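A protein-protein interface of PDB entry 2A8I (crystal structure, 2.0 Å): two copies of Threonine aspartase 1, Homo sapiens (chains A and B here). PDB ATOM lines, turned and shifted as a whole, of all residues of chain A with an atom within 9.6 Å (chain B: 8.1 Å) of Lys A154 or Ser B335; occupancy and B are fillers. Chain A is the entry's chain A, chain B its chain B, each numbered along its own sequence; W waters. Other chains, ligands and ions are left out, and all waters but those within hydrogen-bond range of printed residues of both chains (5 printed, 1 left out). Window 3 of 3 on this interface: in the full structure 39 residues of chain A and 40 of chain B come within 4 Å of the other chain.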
ATOM      1  N   ASP A 121      25.475  -4.163 -19.638  1.00  0.00           N
ATOM      2  CA  ASP A 121      26.819  -4.733 -19.745  1.00  0.00           C
ATOM      3  C   ASP A 121      26.959  -5.888 -18.758  1.00  0.00           C
ATOM      4  O   ASP A 121      26.832  -5.692 -17.558  1.00  0.00           O
ATOM      5  CB  ASP A 121      27.861  -3.656 -19.429  1.00  0.00           C
ATOM      6  CG  ASP A 121      29.284  -4.173 -19.517  1.00  0.00           C
ATOM      7  OD1 ASP A 121      29.669  -4.704 -20.582  1.00  0.00           O
ATOM      8  OD2 ASP A 121      30.023  -4.041 -18.522  1.00  0.00           O
ATOM      9  N   GLY A 122      27.227  -7.085 -19.265  1.00  0.00           N
ATOM     10  CA  GLY A 122      27.350  -8.242 -18.400  1.00  0.00           C
ATOM     11  C   GLY A 122      28.535  -8.230 -17.445  1.00  0.00           C
ATOM     12  O   GLY A 122      28.461  -8.795 -16.353  1.00  0.00           O
ATOM     13  N   LYS A 123      29.628  -7.588 -17.843  1.00  0.00           N
ATOM     14  CA  LYS A 123      30.810  -7.552 -16.994  1.00  0.00           C
ATOM     15  C   LYS A 123      30.611  -6.645 -15.780  1.00  0.00           C
ATOM     16  O   LYS A 123      30.839  -7.056 -14.642  1.00  0.00           O
ATOM     17  CB  LYS A 123      32.019  -7.070 -17.793  1.00  0.00           C
ATOM     18  CG  LYS A 123      33.368  -7.377 -17.145  1.00  0.00           C
ATOM     19  CD  LYS A 123      34.497  -6.671 -17.902  1.00  0.00           C
ATOM     20  CE  LYS A 123      35.864  -7.293 -17.625  1.00  0.00           C
ATOM     21  NZ  LYS A 123      36.156  -7.428 -16.176  1.00  0.00           N
ATOM     22  N   SER A 124      30.179  -5.416 -16.031  1.00  0.00           N
ATOM     23  CA  SER A 124      29.970  -4.438 -14.965  1.00  0.00           C
ATOM     24  C   SER A 124      28.568  -4.477 -14.379  1.00  0.00           C
ATOM     25  O   SER A 124      28.324  -3.913 -13.309  1.00  0.00           O
ATOM     26  CB  SER A 124      30.236  -3.029 -15.495  1.00  0.00           C
ATOM     27  OG  SER A 124      29.223  -2.628 -16.410  1.00  0.00           O
ATOM     28  N   LEU A 125      27.654  -5.131 -15.094  1.00  0.00           N
ATOM     29  CA  LEU A 125      26.257  -5.240 -14.689  1.00  0.00           C
ATOM     30  C   LEU A 125      25.588  -3.877 -14.724  1.00  0.00           C
ATOM     31  O   LEU A 125      24.461  -3.716 -14.249  1.00  0.00           O
ATOM     32  CB  LEU A 125      26.137  -5.839 -13.285  1.00  0.00           C
ATOM     33  CG  LEU A 125      26.698  -7.247 -13.107  1.00  0.00           C
ATOM     34  CD1 LEU A 125      26.478  -7.702 -11.663  1.00  0.00           C
ATOM     35  CD2 LEU A 125      26.020  -8.192 -14.087  1.00  0.00           C
ATOM     36  N   ASN A 126      26.272  -2.893 -15.299  1.00  0.00           N
ATOM     37  CA  ASN A 126      25.697  -1.558 -15.376  1.00  0.00           C
ATOM     38  C   ASN A 126      24.644  -1.474 -16.467  1.00  0.00           C
ATOM     39  O   ASN A 126      24.634  -2.270 -17.410  1.00  0.00           O
ATOM     40  CB  ASN A 126      26.783  -0.502 -15.576  1.00  0.00           C
ATOM     41  CG  ASN A 126      26.554   0.724 -14.705  1.00  0.00           C
ATOM     42  OD1 ASN A 126      27.500   1.402 -14.305  1.00  0.00           O
ATOM     43  ND2 ASN A 126      25.284   1.010 -14.404  1.00  0.00           N
ATOM     44  N   PHE A 127      23.776  -0.480 -16.340  1.00  0.00           N
ATOM     45  CA  PHE A 127      22.640  -0.306 -17.230  1.00  0.00           C
ATOM     46  C   PHE A 127      22.458   1.149 -17.674  1.00  0.00           C
ATOM     47  O   PHE A 127      22.893   2.069 -16.987  1.00  0.00           O
ATOM     48  CB  PHE A 127      21.416  -0.790 -16.442  1.00  0.00           C
ATOM     49  CG  PHE A 127      20.102  -0.583 -17.123  1.00  0.00           C
ATOM     50  CD1 PHE A 127      19.697  -1.423 -18.150  1.00  0.00           C
ATOM     51  CD2 PHE A 127      19.228   0.410 -16.678  1.00  0.00           C
ATOM     52  CE1 PHE A 127      18.436  -1.287 -18.726  1.00  0.00           C
ATOM     53  CE2 PHE A 127      17.971   0.559 -17.243  1.00  0.00           C
ATOM     54  CZ  PHE A 127      17.569  -0.294 -18.270  1.00  0.00           C
ATOM     55  N   LEU A 146      24.819   6.849 -21.153  1.00  0.00           N
ATOM     56  CA  LEU A 146      24.440   6.907 -19.749  1.00  0.00           C
ATOM     57  C   LEU A 146      25.162   5.766 -19.039  1.00  0.00           C
ATOM     58  O   LEU A 146      25.624   5.914 -17.904  1.00  0.00           O
ATOM     59  CB  LEU A 146      22.922   6.754 -19.582  1.00  0.00           C
ATOM     60  CG  LEU A 146      22.045   7.982 -19.854  1.00  0.00           C
ATOM     61  CD1 LEU A 146      20.572   7.588 -19.856  1.00  0.00           C
ATOM     62  CD2 LEU A 146      22.304   9.036 -18.780  1.00  0.00           C
ATOM     63  N   LEU A 147      25.263   4.627 -19.721  1.00  0.00           N
ATOM     64  CA  LEU A 147      25.930   3.452 -19.169  1.00  0.00           C
ATOM     65  C   LEU A 147      27.409   3.765 -18.967  1.00  0.00           C
ATOM     66  O   LEU A 147      27.972   3.484 -17.903  1.00  0.00           O
ATOM     67  CB  LEU A 147      25.759   2.248 -20.112  1.00  0.00           C
ATOM     68  CG  LEU A 147      26.104   0.839 -19.607  1.00  0.00           C
ATOM     69  CD1 LEU A 147      25.597  -0.188 -20.616  1.00  0.00           C
ATOM     70  CD2 LEU A 147      27.614   0.675 -19.410  1.00  0.00           C
ATOM     71  N   CYS A 148      28.034   4.346 -19.990  1.00  0.00           N
ATOM     72  CA  CYS A 148      29.449   4.717 -19.923  1.00  0.00           C
ATOM     73  C   CYS A 148      29.740   5.658 -18.756  1.00  0.00           C
ATOM     74  O   CYS A 148      30.676   5.434 -17.984  1.00  0.00           O
ATOM     75  CB  CYS A 148      29.888   5.378 -21.231  1.00  0.00           C
ATOM     76  SG  CYS A 148      29.941   4.237 -22.628  1.00  0.00           S
ATOM     77  N   GLU A 149      28.940   6.714 -18.634  1.00  0.00           N
ATOM     78  CA  GLU A 149      29.110   7.674 -17.547  1.00  0.00           C
ATOM     79  C   GLU A 149      28.946   6.973 -16.203  1.00  0.00           C
ATOM     80  O   GLU A 149      29.685   7.244 -15.253  1.00  0.00           O
ATOM     81  CB  GLU A 149      28.081   8.801 -17.665  1.00  0.00           C
ATOM     82  CG  GLU A 149      28.284   9.703 -18.867  1.00  0.00           C
ATOM     83  CD  GLU A 149      29.659  10.341 -18.883  1.00  0.00           C
ATOM     84  OE1 GLU A 149      30.125  10.769 -17.803  1.00  0.00           O
ATOM     85  OE2 GLU A 149      30.270  10.421 -19.974  1.00  0.00           O
ATOM     86  N   GLY A 150      27.973   6.069 -16.131  1.00  0.00           N
ATOM     87  CA  GLY A 150      27.735   5.325 -14.906  1.00  0.00           C
ATOM     88  C   GLY A 150      28.979   4.566 -14.489  1.00  0.00           C
ATOM     89  O   GLY A 150      29.260   4.431 -13.299  1.00  0.00           O
ATOM     90  N   GLN A 151      29.722   4.056 -15.468  1.00  0.00           N
ATOM     91  CA  GLN A 151      30.956   3.330 -15.186  1.00  0.00           C
ATOM     92  C   GLN A 151      32.005   4.298 -14.629  1.00  0.00           C
ATOM     93  O   GLN A 151      32.795   3.930 -13.761  1.00  0.00           O
ATOM     94  CB  GLN A 151      31.498   2.668 -16.458  1.00  0.00           C
ATOM     95  CG  GLN A 151      30.878   1.313 -16.776  1.00  0.00           C
ATOM     96  CD  GLN A 151      30.928   0.379 -15.588  1.00  0.00           C
ATOM     97  OE1 GLN A 151      30.090   0.459 -14.686  1.00  0.00           O
ATOM     98  NE2 GLN A 151      31.924  -0.505 -15.568  1.00  0.00           N
ATOM     99  N   LYS A 152      32.009   5.531 -15.137  1.00  0.00           N
ATOM    100  CA  LYS A 152      32.945   6.549 -14.674  1.00  0.00           C
ATOM    101  C   LYS A 152      32.642   6.914 -13.230  1.00  0.00           C
ATOM    102  O   LYS A 152      33.534   7.298 -12.479  1.00  0.00           O
ATOM    103  CB  LYS A 152      32.844   7.811 -15.531  1.00  0.00           C
ATOM    104  CG  LYS A 152      33.471   7.701 -16.913  1.00  0.00           C
ATOM    105  CD  LYS A 152      33.393   9.050 -17.618  1.00  0.00           C
ATOM    106  CE  LYS A 152      33.817   8.961 -19.077  1.00  0.00           C
ATOM    107  NZ  LYS A 152      33.600  10.266 -19.779  1.00  0.00           N
ATOM    108  N   GLY A 153      31.375   6.791 -12.849  1.00  0.00           N
ATOM    109  CA  GLY A 153      30.978   7.114 -11.493  1.00  0.00           C
ATOM    110  C   GLY A 153      31.430   6.116 -10.441  1.00  0.00           C
ATOM    111  O   GLY A 153      31.434   6.432  -9.251  1.00  0.00           O
ATOM    112  N   LYS A 154      31.814   4.913 -10.861  1.00  0.00           N
ATOM    113  CA  LYS A 154      32.248   3.891  -9.910  1.00  0.00           C
ATOM    114  C   LYS A 154      33.651   4.147  -9.379  1.00  0.00           C
ATOM    115  O   LYS A 154      33.966   3.806  -8.233  1.00  0.00           O
ATOM    116  CB  LYS A 154      32.174   2.503 -10.547  1.00  0.00           C
ATOM    117  CG  LYS A 154      30.747   2.003 -10.740  1.00  0.00           C
ATOM    118  CD  LYS A 154      30.728   0.611 -11.342  1.00  0.00           C
ATOM    119  CE  LYS A 154      29.307   0.074 -11.436  1.00  0.00           C
ATOM    120  NZ  LYS A 154      29.286  -1.315 -11.995  1.00  0.00           N
ATOM    121  N   LEU A 155      34.495   4.746 -10.216  1.00  0.00           N
ATOM    122  CA  LEU A 155      35.856   5.068  -9.819  1.00  0.00           C
ATOM    123  C   LEU A 155      35.780   6.323  -8.964  1.00  0.00           C
ATOM    124  O   LEU A 155      36.377   7.358  -9.279  1.00  0.00           O
ATOM    125  CB  LEU A 155      36.732   5.307 -11.052  1.00  0.00           C
ATOM    126  CG  LEU A 155      36.956   4.080 -11.943  1.00  0.00           C
ATOM    127  CD1 LEU A 155      35.637   3.623 -12.534  1.00  0.00           C
ATOM    128  CD2 LEU A 155      37.932   4.428 -13.059  1.00  0.00           C
ATOM    129  N   SER A 156      35.020   6.213  -7.879  1.00  0.00           N
ATOM    130  CA  SER A 156      34.827   7.312  -6.951  1.00  0.00           C
ATOM    131  C   SER A 156      34.413   8.570  -7.711  1.00  0.00           C
ATOM    132  O   SER A 156      35.245   9.290  -8.275  1.00  0.00           O
ATOM    133  CB  SER A 156      36.115   7.545  -6.150  1.00  0.00           C
ATOM    134  OG  SER A 156      36.474   6.376  -5.418  1.00  0.00           O
ATOM    135  N   ALA A 157      33.108   8.813  -7.741  1.00  0.00           N
ATOM    136  CA  ALA A 157      32.558   9.975  -8.427  1.00  0.00           C
ATOM    137  C   ALA A 157      31.195  10.293  -7.834  1.00  0.00           C
ATOM    138  O   ALA A 157      30.156  10.012  -8.451  1.00  0.00           O
ATOM    139  CB  ALA A 157      32.431   9.700  -9.923  1.00  0.00           C
ATOM    140  N   GLY A 158      31.212  10.866  -6.631  1.00  0.00           N
ATOM    141  CA  GLY A 158      29.980  11.229  -5.949  1.00  0.00           C
ATOM    142  C   GLY A 158      28.917  10.145  -5.992  1.00  0.00           C
ATOM    143  O   GLY A 158      29.223   8.958  -6.149  1.00  0.00           O
ATOM    144  N   ARG A 159      27.660  10.551  -5.849  1.00  0.00           N
ATOM    145  CA  ARG A 159      26.565   9.593  -5.870  1.00  0.00           C
ATOM    146  C   ARG A 159      26.410   9.020  -7.273  1.00  0.00           C
ATOM    147  O   ARG A 159      26.782   9.658  -8.260  1.00  0.00           O
ATOM    148  CB  ARG A 159      25.265  10.270  -5.449  1.00  0.00           C
ATOM    149  CG  ARG A 159      24.693  11.184  -6.508  1.00  0.00           C
ATOM    150  CD  ARG A 159      23.624  12.052  -5.895  1.00  0.00           C
ATOM    151  NE  ARG A 159      22.966  12.879  -6.892  1.00  0.00           N
ATOM    152  CZ  ARG A 159      22.081  13.822  -6.600  1.00  0.00           C
ATOM    153  NH1 ARG A 159      21.756  14.055  -5.332  1.00  0.00           N
ATOM    154  NH2 ARG A 159      21.521  14.526  -7.575  1.00  0.00           N
ATOM    155  N   ILE A 160      25.848   7.820  -7.351  1.00  0.00           N
ATOM    156  CA  ILE A 160      25.644   7.140  -8.623  1.00  0.00           C
ATOM    157  C   ILE A 160      24.954   8.030  -9.655  1.00  0.00           C
ATOM    158  O   ILE A 160      23.946   8.679  -9.361  1.00  0.00           O
ATOM    159  CB  ILE A 160      24.787   5.868  -8.443  1.00  0.00           C
ATOM    160  CG1 ILE A 160      25.375   4.993  -7.335  1.00  0.00           C
ATOM    161  CG2 ILE A 160      24.749   5.086  -9.750  1.00  0.00           C
ATOM    162  CD1 ILE A 160      24.473   3.829  -6.919  1.00  0.00           C
ATOM    163  N   PRO A 161      25.506   8.084 -10.880  1.00  0.00           N
ATOM    164  CA  PRO A 161      24.931   8.896 -11.960  1.00  0.00           C
ATOM    165  C   PRO A 161      23.587   8.287 -12.382  1.00  0.00           C
ATOM    166  O   PRO A 161      23.274   7.143 -12.033  1.00  0.00           O
ATOM    167  CB  PRO A 161      25.974   8.786 -13.073  1.00  0.00           C
ATOM    168  CG  PRO A 161      27.255   8.527 -12.329  1.00  0.00           C
ATOM    169  CD  PRO A 161      26.816   7.541 -11.274  1.00  0.00           C
ATOM    170  N   HIS B 296      20.078   1.652  -5.655  1.00  0.00           N
ATOM    171  CA  HIS B 296      20.287   0.352  -5.022  1.00  0.00           C
ATOM    172  C   HIS B 296      19.065  -0.544  -5.165  1.00  0.00           C
ATOM    173  O   HIS B 296      19.199  -1.736  -5.445  1.00  0.00           O
ATOM    174  CB  HIS B 296      20.607   0.516  -3.533  1.00  0.00           C
ATOM    175  CG  HIS B 296      21.856   1.293  -3.260  1.00  0.00           C
ATOM    176  ND1 HIS B 296      22.230   1.673  -1.989  1.00  0.00           N
ATOM    177  CD2 HIS B 296      22.818   1.760  -4.090  1.00  0.00           C
ATOM    178  CE1 HIS B 296      23.368   2.341  -2.047  1.00  0.00           C
ATOM    179  NE2 HIS B 296      23.747   2.406  -3.310  1.00  0.00           N
ATOM    180  N   ARG B 299      18.624  -1.656  -9.139  1.00  0.00           N
ATOM    181  CA  ARG B 299      19.552  -2.671  -9.633  1.00  0.00           C
ATOM    182  C   ARG B 299      19.245  -4.065  -9.110  1.00  0.00           C
ATOM    183  O   ARG B 299      19.516  -5.048  -9.785  1.00  0.00           O
ATOM    184  CB  ARG B 299      21.002  -2.307  -9.294  1.00  0.00           C
ATOM    185  CG  ARG B 299      21.444  -0.922  -9.737  1.00  0.00           C
ATOM    186  CD  ARG B 299      20.930  -0.573 -11.125  1.00  0.00           C
ATOM    187  NE  ARG B 299      21.483   0.699 -11.584  1.00  0.00           N
ATOM    188  CZ  ARG B 299      22.653   0.822 -12.206  1.00  0.00           C
ATOM    189  NH1 ARG B 299      23.395  -0.253 -12.451  1.00  0.00           N
ATOM    190  NH2 ARG B 299      23.087   2.022 -12.570  1.00  0.00           N
ATOM    191  N   SER B 330      24.548  -8.241  -2.767  1.00  0.00           N
ATOM    192  CA  SER B 330      24.230  -8.411  -4.186  1.00  0.00           C
ATOM    193  C   SER B 330      25.390  -8.050  -5.124  1.00  0.00           C
ATOM    194  O   SER B 330      26.014  -6.998  -4.980  1.00  0.00           O
ATOM    195  CB  SER B 330      23.017  -7.550  -4.555  1.00  0.00           C
ATOM    196  OG  SER B 330      22.938  -7.346  -5.959  1.00  0.00           O
ATOM    197  N   PRO B 331      25.698  -8.927  -6.095  1.00  0.00           N
ATOM    198  CA  PRO B 331      26.783  -8.659  -7.049  1.00  0.00           C
ATOM    199  C   PRO B 331      26.494  -7.360  -7.816  1.00  0.00           C
ATOM    200  O   PRO B 331      27.403  -6.690  -8.314  1.00  0.00           O
ATOM    201  CB  PRO B 331      26.736  -9.873  -7.975  1.00  0.00           C
ATOM    202  CG  PRO B 331      26.270 -10.965  -7.073  1.00  0.00           C
ATOM    203  CD  PRO B 331      25.181 -10.299  -6.257  1.00  0.00           C
ATOM    204  N   PHE B 332      25.215  -7.009  -7.905  1.00  0.00           N
ATOM    205  CA  PHE B 332      24.809  -5.807  -8.617  1.00  0.00           C
ATOM    206  C   PHE B 332      25.134  -4.514  -7.881  1.00  0.00           C
ATOM    207  O   PHE B 332      24.966  -3.424  -8.427  1.00  0.00           O
ATOM    208  CB  PHE B 332      23.308  -5.866  -8.936  1.00  0.00           C
ATOM    209  CG  PHE B 332      22.957  -6.904  -9.957  1.00  0.00           C
ATOM    210  CD1 PHE B 332      22.934  -8.252  -9.618  1.00  0.00           C
ATOM    211  CD2 PHE B 332      22.723  -6.542 -11.279  1.00  0.00           C
ATOM    212  CE1 PHE B 332      22.687  -9.227 -10.580  1.00  0.00           C
ATOM    213  CE2 PHE B 332      22.475  -7.510 -12.250  1.00  0.00           C
ATOM    214  CZ  PHE B 332      22.458  -8.854 -11.897  1.00  0.00           C
ATOM    215  N   LEU B 333      25.606  -4.632  -6.648  1.00  0.00           N
ATOM    216  CA  LEU B 333      25.946  -3.456  -5.858  1.00  0.00           C
ATOM    217  C   LEU B 333      27.344  -3.590  -5.258  1.00  0.00           C
ATOM    218  O   LEU B 333      27.706  -2.854  -4.342  1.00  0.00           O
ATOM    219  CB  LEU B 333      24.919  -3.269  -4.739  1.00  0.00           C
ATOM    220  CG  LEU B 333      23.474  -3.042  -5.198  1.00  0.00           C
ATOM    221  CD1 LEU B 333      22.555  -3.001  -3.990  1.00  0.00           C
ATOM    222  CD2 LEU B 333      23.381  -1.743  -5.989  1.00  0.00           C
ATOM    223  N   ALA B 334      28.123  -4.529  -5.788  1.00  0.00           N
ATOM    224  CA  ALA B 334      29.476  -4.781  -5.297  1.00  0.00           C
ATOM    225  C   ALA B 334      30.393  -3.558  -5.293  1.00  0.00           C
ATOM    226  O   ALA B 334      31.211  -3.402  -4.386  1.00  0.00           O
ATOM    227  CB  ALA B 334      30.114  -5.906  -6.106  1.00  0.00           C
ATOM    228  N   SER B 335      30.261  -2.695  -6.298  1.00  0.00           N
ATOM    229  CA  SER B 335      31.099  -1.501  -6.397  1.00  0.00           C
ATOM    230  C   SER B 335      30.746  -0.404  -5.398  1.00  0.00           C
ATOM    231  O   SER B 335      31.457   0.595  -5.293  1.00  0.00           O
ATOM    232  CB  SER B 335      31.030  -0.915  -7.808  1.00  0.00           C
ATOM    233  OG  SER B 335      31.624  -1.794  -8.749  1.00  0.00           O
ATOM    234  N   GLU B 336      29.653  -0.587  -4.668  1.00  0.00           N
ATOM    235  CA  GLU B 336      29.226   0.417  -3.713  1.00  0.00           C
ATOM    236  C   GLU B 336      29.741   0.151  -2.303  1.00  0.00           C
ATOM    237  O   GLU B 336      29.905  -0.995  -1.882  1.00  0.00           O
ATOM    238  CB  GLU B 336      27.695   0.519  -3.699  1.00  0.00           C
ATOM    239  CG  GLU B 336      27.079   0.898  -5.050  1.00  0.00           C
ATOM    240  CD  GLU B 336      27.763   2.108  -5.677  1.00  0.00           C
ATOM    241  OE1 GLU B 336      27.909   3.131  -4.978  1.00  0.00           O
ATOM    242  OE2 GLU B 336      28.156   2.040  -6.863  1.00  0.00           O
ATOM    243  N   ASP B 337      30.010   1.231  -1.585  1.00  0.00           N
ATOM    244  CA  ASP B 337      30.489   1.144  -0.215  1.00  0.00           C
ATOM    245  C   ASP B 337      29.291   1.409   0.682  1.00  0.00           C
ATOM    246  O   ASP B 337      29.070   2.534   1.133  1.00  0.00           O
ATOM    247  CB  ASP B 337      31.602   2.178   0.020  1.00  0.00           C
ATOM    248  CG  ASP B 337      31.366   3.477  -0.733  1.00  0.00           C
ATOM    249  OD1 ASP B 337      32.324   4.283  -0.840  1.00  0.00           O
ATOM    250  OD2 ASP B 337      30.227   3.699  -1.216  1.00  0.00           O
ATOM    251  N   GLY B 338      28.513   0.356   0.918  1.00  0.00           N
ATOM    252  CA  GLY B 338      27.324   0.475   1.738  1.00  0.00           C
ATOM    253  C   GLY B 338      26.085   0.470   0.863  1.00  0.00           C
ATOM    254  O   GLY B 338      26.002   1.210  -0.119  1.00  0.00           O
ATOM    255  N   VAL B 339      25.128  -0.381   1.206  1.00  0.00           N
ATOM    256  CA  VAL B 339      23.877  -0.488   0.460  1.00  0.00           C
ATOM    257  C   VAL B 339      22.780   0.070   1.371  1.00  0.00           C
ATOM    258  O   VAL B 339      22.663  -0.328   2.530  1.00  0.00           O
ATOM    259  CB  VAL B 339      23.608  -1.963   0.084  1.00  0.00           C
ATOM    260  CG1 VAL B 339      22.238  -2.106  -0.566  1.00  0.00           C
ATOM    261  CG2 VAL B 339      24.696  -2.445  -0.874  1.00  0.00           C
HETATM  262  O   HOH W   1      30.023  -3.647 -10.434  1.00  0.00           O
HETATM  263  O   HOH W   2      24.555   4.736 -13.066  1.00  0.00           O
HETATM  264  O   HOH W   3      22.462  -3.155 -12.607  1.00  0.00           O
HETATM  265  O   HOH W   4      29.046   4.258  -8.385  1.00  0.00           O
HETATM  266  O   HOH W   5      24.849  -2.568 -11.183  1.00  0.00           O
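The guanidinium group (NH1) of Arg B299 sits close to the side-chain amide nitrogen (ND2) of Asn A126 (3.0 Å).
The side-chain amide oxygen (OE1) of Gln A151 lies close to the side-chain amide oxygen (OD1) of Asn A126 (2.8 Å).
OG of Ser A124 lies close to N of Asn A126, 3.2 Å away.
The side-chain amide oxygen (OE1) of Gln A151 is in hydrogen-bond range of the side-chain amino group (NZ) of Lys A154 (3.3 Å).
The backbone NH (N) of Phe B332 sits close to the side-chain hydroxyl (OG) of Ser B330.
NZ of Lys A154 is in hydrogen-bond range of O of Ser A124 (3.1 Å).
N of Asp A121 is in hydrogen-bond range of O of Asn A126 (3.0 Å).
Leu A125 touches Pro B331.
Leu A125 touches Phe B332.
Phe A127 touches Arg B299.
Ser B335 touches Lys A154.
Ile A160 touches His B296.
Ile A160 touches Glu B336.
Printed residues of chain B within 4 Å of Phe A127: Arg B299 (3.9 Å).
No residue of chain B comes within 4 Å of Gly A153.
Lys A154 touches just one residue of chain B: Ser B335.
Of the printed residues of chain B, Ile A160 touches His B296 and Glu B336.
Pro A161 touches none of the printed residues of chain B.
Of the printed residues of chain A, Arg B299 touches Asn A126 and Phe A127.
Of the printed residues of chain A, Pro B331 touches Leu A125.
Printed residues of chain A within 4 Å of Phe B332: Leu A125.
No residue of chain A comes within 4 Å of Ala B334.
Ser B335 touches just one residue of chain A: Lys A154 (3.6 Å).
Of chain A, only Ile A160 (3.9 Å) comes within 4 Å of Glu B336.
Printed residues of chain B that touch a printed residue of chain A: His B296, Arg B299, Pro B331, Phe B332, Ser B335 and Glu B336.
Printed residues of chain A that touch a printed residue of chain B: Leu A125, Asn A126, Phe A127, Lys A154 and Ile A160.
Hydrophobic or aromatic side chains of chain A that line the printed part of chain B: Leu A125 and Ile A160.
No position is printed for both chains.
Of the 7 pairs that touch across the chains among the printed residues, none has its exchanged pair printed and touching as well.
Water W3 lies within hydrogen-bond range of the backbone carbonyl oxygen (O) of Leu A125 (2.6 Å) and the guanidinium group (NH1) of Arg B299 (3.1 Å).
Water W4 bridges the side-chain carboxylate of Glu B336 (2.8 Å) and the backbone carbonyl oxygen of Gly A153 (3.3 Å).
Water W5 lies within hydrogen-bond range of O of Phe B332 (2.9 Å), NH1 of Arg B299 (3.0 Å) and O of Leu A125 (3.3 Å).
Water W1 lies within hydrogen-bond range of the side-chain amino group (NZ) of Lys A154 (2.9 Å), the side-chain hydroxyl (OG) of Ser B335 (3.0 Å) and the backbone carbonyl oxygen (O) of Ser A124 (3.4 Å).
Water W2 lies within hydrogen-bond range of O of Pro A161 (2.9 Å) and NH2 of Arg B299 (3.1 Å).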
